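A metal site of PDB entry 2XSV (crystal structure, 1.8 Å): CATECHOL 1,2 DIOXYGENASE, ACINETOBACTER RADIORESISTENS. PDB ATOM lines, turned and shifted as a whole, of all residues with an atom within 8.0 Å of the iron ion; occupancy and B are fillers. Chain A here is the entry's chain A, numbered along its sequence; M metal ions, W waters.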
ATOM      1  N   ILE A 107      18.845  13.901  31.569  1.00  0.00           N
ATOM      2  CA  ILE A 107      18.697  13.027  30.383  1.00  0.00           C
ATOM      3  C   ILE A 107      17.884  13.665  29.264  1.00  0.00           C
ATOM      4  O   ILE A 107      16.968  14.480  29.523  1.00  0.00           O
ATOM      5  CB  ILE A 107      18.124  11.608  30.732  1.00  0.00           C
ATOM      6  CG1 ILE A 107      16.595  11.660  31.043  1.00  0.00           C
ATOM      7  CG2 ILE A 107      18.985  10.928  31.850  1.00  0.00           C
ATOM      8  CD1 ILE A 107      15.952  10.250  31.307  1.00  0.00           C
ATOM      9  N   GLU A 108      18.266  13.308  28.038  1.00  0.00           N
ATOM     10  CA  GLU A 108      17.533  13.696  26.840  1.00  0.00           C
ATOM     11  C   GLU A 108      16.166  13.003  26.731  1.00  0.00           C
ATOM     12  O   GLU A 108      15.186  13.620  26.278  1.00  0.00           O
ATOM     13  CB  GLU A 108      18.373  13.333  25.596  1.00  0.00           C
ATOM     14  CG  GLU A 108      17.829  13.868  24.257  1.00  0.00           C
ATOM     15  CD  GLU A 108      18.769  13.527  23.092  1.00  0.00           C
ATOM     16  OE1 GLU A 108      20.013  13.567  23.258  1.00  0.00           O
ATOM     17  OE2 GLU A 108      18.258  13.195  21.992  1.00  0.00           O
ATOM     18  N   GLY A 109      16.120  11.735  27.089  1.00  0.00           N
ATOM     19  CA  GLY A 109      14.984  10.882  26.741  1.00  0.00           C
ATOM     20  C   GLY A 109      14.951  10.569  25.253  1.00  0.00           C
ATOM     21  O   GLY A 109      15.809  11.058  24.475  1.00  0.00           O
ATOM     22  N   PRO A 110      13.986   9.739  24.824  1.00  0.00           N
ATOM     23  CA  PRO A 110      14.046   9.223  23.469  1.00  0.00           C
ATOM     24  C   PRO A 110      13.150   9.970  22.473  1.00  0.00           C
ATOM     25  O   PRO A 110      13.012   9.494  21.339  1.00  0.00           O
ATOM     26  CB  PRO A 110      13.537   7.787  23.649  1.00  0.00           C
ATOM     27  CG  PRO A 110      12.480   7.927  24.713  1.00  0.00           C
ATOM     28  CD  PRO A 110      13.057   8.960  25.678  1.00  0.00           C
ATOM     29  N   LEU A 111      12.609  11.130  22.851  1.00  0.00           N
ATOM     30  CA  LEU A 111      11.547  11.751  22.037  1.00  0.00           C
ATOM     31  C   LEU A 111      11.859  13.108  21.375  1.00  0.00           C
ATOM     32  O   LEU A 111      10.924  13.845  20.976  1.00  0.00           O
ATOM     33  CB  LEU A 111      10.250  11.855  22.860  1.00  0.00           C
ATOM     34  CG  LEU A 111       9.735  10.582  23.486  1.00  0.00           C
ATOM     35  CD1 LEU A 111       8.492  10.873  24.283  1.00  0.00           C
ATOM     36  CD2 LEU A 111       9.481   9.435  22.443  1.00  0.00           C
ATOM     37  N   TYR A 112      13.141  13.447  21.229  1.00  0.00           N
ATOM     38  CA  TYR A 112      13.506  14.640  20.462  1.00  0.00           C
ATOM     39  C   TYR A 112      13.227  14.402  18.980  1.00  0.00           C
ATOM     40  O   TYR A 112      13.394  13.266  18.479  1.00  0.00           O
ATOM     41  CB  TYR A 112      14.991  14.978  20.642  1.00  0.00           C
ATOM     42  CG  TYR A 112      15.484  16.146  19.785  1.00  0.00           C
ATOM     43  CD1 TYR A 112      15.146  17.477  20.101  1.00  0.00           C
ATOM     44  CD2 TYR A 112      16.264  15.905  18.646  1.00  0.00           C
ATOM     45  CE1 TYR A 112      15.614  18.526  19.327  1.00  0.00           C
ATOM     46  CE2 TYR A 112      16.718  16.958  17.858  1.00  0.00           C
ATOM     47  CZ  TYR A 112      16.385  18.255  18.189  1.00  0.00           C
ATOM     48  OH  TYR A 112      16.860  19.283  17.418  1.00  0.00           O
ATOM     49  N   TRP A 159      10.922  20.858  23.954  1.00  0.00           N
ATOM     50  CA  TRP A 159       9.815  19.984  23.558  1.00  0.00           C
ATOM     51  C   TRP A 159       9.157  19.410  24.818  1.00  0.00           C
ATOM     52  O   TRP A 159       9.818  19.248  25.825  1.00  0.00           O
ATOM     53  CB  TRP A 159      10.290  18.884  22.555  1.00  0.00           C
ATOM     54  CG  TRP A 159      11.337  17.848  23.103  1.00  0.00           C
ATOM     55  CD1 TRP A 159      11.100  16.558  23.389  1.00  0.00           C
ATOM     56  CD2 TRP A 159      12.769  18.033  23.288  1.00  0.00           C
ATOM     57  NE1 TRP A 159      12.264  15.909  23.781  1.00  0.00           N
ATOM     58  CE2 TRP A 159      13.303  16.800  23.760  1.00  0.00           C
ATOM     59  CE3 TRP A 159      13.631  19.140  23.180  1.00  0.00           C
ATOM     60  CZ2 TRP A 159      14.669  16.620  24.085  1.00  0.00           C
ATOM     61  CZ3 TRP A 159      15.011  18.977  23.523  1.00  0.00           C
ATOM     62  CH2 TRP A 159      15.502  17.713  23.945  1.00  0.00           C
ATOM     63  N   HIS A 160       7.835  19.154  24.765  1.00  0.00           N
ATOM     64  CA  HIS A 160       7.123  18.648  25.952  1.00  0.00           C
ATOM     65  C   HIS A 160       5.803  18.049  25.532  1.00  0.00           C
ATOM     66  O   HIS A 160       5.389  18.197  24.373  1.00  0.00           O
ATOM     67  CB  HIS A 160       6.965  19.751  27.053  1.00  0.00           C
ATOM     68  CG  HIS A 160       5.996  20.851  26.728  1.00  0.00           C
ATOM     69  ND1 HIS A 160       4.612  20.698  26.775  1.00  0.00           N
ATOM     70  CD2 HIS A 160       6.205  22.155  26.431  1.00  0.00           C
ATOM     71  CE1 HIS A 160       4.026  21.852  26.495  1.00  0.00           C
ATOM     72  NE2 HIS A 160       4.975  22.747  26.265  1.00  0.00           N
ATOM     73  N   ALA A 161       5.172  17.336  26.475  1.00  0.00           N
ATOM     74  CA  ALA A 161       3.939  16.600  26.265  1.00  0.00           C
ATOM     75  C   ALA A 161       2.701  17.505  26.323  1.00  0.00           C
ATOM     76  O   ALA A 161       2.701  18.566  26.969  1.00  0.00           O
ATOM     77  CB  ALA A 161       3.842  15.450  27.289  1.00  0.00           C
ATOM     78  N   GLY A 165      -0.348  13.774  28.137  1.00  0.00           N
ATOM     79  CA  GLY A 165       0.974  13.184  28.326  1.00  0.00           C
ATOM     80  C   GLY A 165       1.599  12.643  27.029  1.00  0.00           C
ATOM     81  O   GLY A 165       2.469  11.780  27.105  1.00  0.00           O
ATOM     82  N   TYR A 167       3.440  13.152  23.046  1.00  0.00           N
ATOM     83  CA  TYR A 167       4.328  14.036  22.286  1.00  0.00           C
ATOM     84  C   TYR A 167       3.975  13.974  20.803  1.00  0.00           C
ATOM     85  O   TYR A 167       3.677  12.894  20.279  1.00  0.00           O
ATOM     86  CB  TYR A 167       5.773  13.538  22.415  1.00  0.00           C
ATOM     87  CG  TYR A 167       6.430  13.871  23.741  1.00  0.00           C
ATOM     88  CD1 TYR A 167       7.345  14.917  23.823  1.00  0.00           C
ATOM     89  CD2 TYR A 167       6.137  13.147  24.902  1.00  0.00           C
ATOM     90  CE1 TYR A 167       7.982  15.243  25.039  1.00  0.00           C
ATOM     91  CE2 TYR A 167       6.787  13.430  26.123  1.00  0.00           C
ATOM     92  CZ  TYR A 167       7.716  14.452  26.172  1.00  0.00           C
ATOM     93  OH  TYR A 167       8.331  14.753  27.361  1.00  0.00           O
ATOM     94  N   VAL A 199       1.672  17.487  31.342  1.00  0.00           N
ATOM     95  CA  VAL A 199       1.381  16.518  32.401  1.00  0.00           C
ATOM     96  C   VAL A 199       2.423  15.381  32.300  1.00  0.00           C
ATOM     97  O   VAL A 199       2.918  15.097  31.207  1.00  0.00           O
ATOM     98  CB  VAL A 199      -0.115  16.032  32.241  1.00  0.00           C
ATOM     99  CG1 VAL A 199      -0.266  15.031  31.129  1.00  0.00           C
ATOM    100  CG2 VAL A 199      -0.617  15.475  33.506  1.00  0.00           C
ATOM    101  N   TYR A 201       3.607  11.351  32.496  1.00  0.00           N
ATOM    102  CA  TYR A 201       3.098  10.252  31.692  1.00  0.00           C
ATOM    103  C   TYR A 201       3.802   8.981  32.029  1.00  0.00           C
ATOM    104  O   TYR A 201       4.874   9.001  32.608  1.00  0.00           O
ATOM    105  CB  TYR A 201       3.355  10.554  30.212  1.00  0.00           C
ATOM    106  CG  TYR A 201       4.767  10.962  29.864  1.00  0.00           C
ATOM    107  CD1 TYR A 201       5.744   9.994  29.552  1.00  0.00           C
ATOM    108  CD2 TYR A 201       5.139  12.318  29.789  1.00  0.00           C
ATOM    109  CE1 TYR A 201       7.034  10.342  29.212  1.00  0.00           C
ATOM    110  CE2 TYR A 201       6.451  12.689  29.432  1.00  0.00           C
ATOM    111  CZ  TYR A 201       7.399  11.694  29.157  1.00  0.00           C
ATOM    112  OH  TYR A 201       8.696  12.043  28.811  1.00  0.00           O
ATOM    113  N   ARG A 222       6.819   9.261  34.691  1.00  0.00           N
ATOM    114  CA  ARG A 222       7.659  10.457  34.840  1.00  0.00           C
ATOM    115  C   ARG A 222       6.821  11.643  35.322  1.00  0.00           C
ATOM    116  O   ARG A 222       5.646  11.769  34.938  1.00  0.00           O
ATOM    117  CB  ARG A 222       8.357  10.876  33.534  1.00  0.00           C
ATOM    118  CG  ARG A 222       8.971   9.734  32.769  1.00  0.00           C
ATOM    119  CD  ARG A 222      10.021  10.233  31.830  1.00  0.00           C
ATOM    120  NE  ARG A 222      11.106  10.850  32.577  1.00  0.00           N
ATOM    121  CZ  ARG A 222      11.992  11.652  32.016  1.00  0.00           C
ATOM    122  NH1 ARG A 222      11.907  11.930  30.686  1.00  0.00           N
ATOM    123  NH2 ARG A 222      12.940  12.178  32.778  1.00  0.00           N
ATOM    124  N   PRO A 223       7.409  12.488  36.204  1.00  0.00           N
ATOM    125  CA  PRO A 223       6.715  13.745  36.573  1.00  0.00           C
ATOM    126  C   PRO A 223       6.666  14.663  35.354  1.00  0.00           C
ATOM    127  O   PRO A 223       7.474  14.488  34.388  1.00  0.00           O
ATOM    128  CB  PRO A 223       7.613  14.350  37.647  1.00  0.00           C
ATOM    129  CG  PRO A 223       9.039  13.845  37.320  1.00  0.00           C
ATOM    130  CD  PRO A 223       8.783  12.430  36.735  1.00  0.00           C
ATOM    131  N   SER A 224       5.777  15.671  35.416  1.00  0.00           N
ATOM    132  CA  SER A 224       5.723  16.695  34.328  1.00  0.00           C
ATOM    133  C   SER A 224       7.084  17.383  34.168  1.00  0.00           C
ATOM    134  O   SER A 224       7.819  17.616  35.178  1.00  0.00           O
ATOM    135  CB  SER A 224       4.685  17.771  34.669  1.00  0.00           C
ATOM    136  OG  SER A 224       5.081  18.387  35.892  1.00  0.00           O
ATOM    137  N   HIS A 225       7.432  17.716  32.919  1.00  0.00           N
ATOM    138  CA  HIS A 225       8.743  18.342  32.666  1.00  0.00           C
ATOM    139  C   HIS A 225       8.731  18.959  31.270  1.00  0.00           C
ATOM    140  O   HIS A 225       7.866  18.646  30.459  1.00  0.00           O
ATOM    141  CB  HIS A 225       9.870  17.267  32.752  1.00  0.00           C
ATOM    142  CG  HIS A 225       9.672  16.118  31.811  1.00  0.00           C
ATOM    143  ND1 HIS A 225       8.867  15.042  32.114  1.00  0.00           N
ATOM    144  CD2 HIS A 225      10.148  15.890  30.549  1.00  0.00           C
ATOM    145  CE1 HIS A 225       8.860  14.191  31.092  1.00  0.00           C
ATOM    146  NE2 HIS A 225       9.641  14.680  30.133  1.00  0.00           N
ATOM    147  N   VAL A 226       9.715  19.821  30.998  1.00  0.00           N
ATOM    148  CA  VAL A 226       9.920  20.387  29.673  1.00  0.00           C
ATOM    149  C   VAL A 226      11.373  20.134  29.362  1.00  0.00           C
ATOM    150  O   VAL A 226      12.246  20.452  30.196  1.00  0.00           O
ATOM    151  CB  VAL A 226       9.581  21.882  29.596  1.00  0.00           C
ATOM    152  CG1 VAL A 226       9.922  22.461  28.196  1.00  0.00           C
ATOM    153  CG2 VAL A 226       8.063  22.097  29.906  1.00  0.00           C
ATOM    154  N   HIS A 227      11.643  19.575  28.188  1.00  0.00           N
ATOM    155  CA  HIS A 227      13.033  19.292  27.776  1.00  0.00           C
ATOM    156  C   HIS A 227      13.709  20.493  27.087  1.00  0.00           C
ATOM    157  O   HIS A 227      13.052  21.265  26.387  1.00  0.00           O
ATOM    158  CB  HIS A 227      13.006  18.175  26.714  1.00  0.00           C
ATOM    159  CG  HIS A 227      12.505  16.852  27.185  1.00  0.00           C
ATOM    160  ND1 HIS A 227      13.335  15.894  27.725  1.00  0.00           N
ATOM    161  CD2 HIS A 227      11.269  16.304  27.152  1.00  0.00           C
ATOM    162  CE1 HIS A 227      12.629  14.815  28.028  1.00  0.00           C
ATOM    163  NE2 HIS A 227      11.369  15.019  27.674  1.00  0.00           N
ATOM    164  N   GLN A 241      16.421  19.727  31.566  1.00  0.00           N
ATOM    165  CA  GLN A 241      14.975  19.915  31.654  1.00  0.00           C
ATOM    166  C   GLN A 241      14.648  20.748  32.891  1.00  0.00           C
ATOM    167  O   GLN A 241      15.533  21.005  33.727  1.00  0.00           O
ATOM    168  CB  GLN A 241      14.264  18.565  31.785  1.00  0.00           C
ATOM    169  CG  GLN A 241      14.352  17.892  33.148  1.00  0.00           C
ATOM    170  CD  GLN A 241      13.739  16.488  33.139  1.00  0.00           C
ATOM    171  OE1 GLN A 241      13.387  15.940  32.076  1.00  0.00           O
ATOM    172  NE2 GLN A 241      13.619  15.903  34.345  1.00  0.00           N
HETATM  173 FE    FE M   1       9.794  13.730  28.198  1.00  0.00          FE
HETATM  174  O   HOH W   1      10.739  12.331  26.712  1.00  0.00           O
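The backbone NH of His 227 lies within hydrogen-bond range of the backbone carbonyl oxygen of Trp 159, at 3.0 Å. A ring nitrogen (ND1) of His 227 is in hydrogen-bond range of the backbone carbonyl oxygen of Glu 108, at 3.3 Å. ND1 of His 225 is in hydrogen-bond range of O of Pro 223, at 2.7 Å. N of Arg 222 sits at hydrogen-bond distance from O of Tyr 201.
The iron ion is bound by OH of Tyr 167 (2.0 Å). The iron ion is bound by a ring nitrogen (NE2) of His 227 (2.1 Å). The iron ion is bound by OH of Tyr 201. NE2 of His 225 is bound to the iron ion. The iron ion is bound by water W1, 2.2 Å away.
Arg 222 touches the iron ion (NH1 to FE, 3.7 Å). Five residues have an atom within 4 Å of the iron ion: Tyr 167, Tyr 201, Arg 222, His 225 and His 227. The nearest printed residue that does not touch the iron ion is Leu 111 (5.0 Å).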
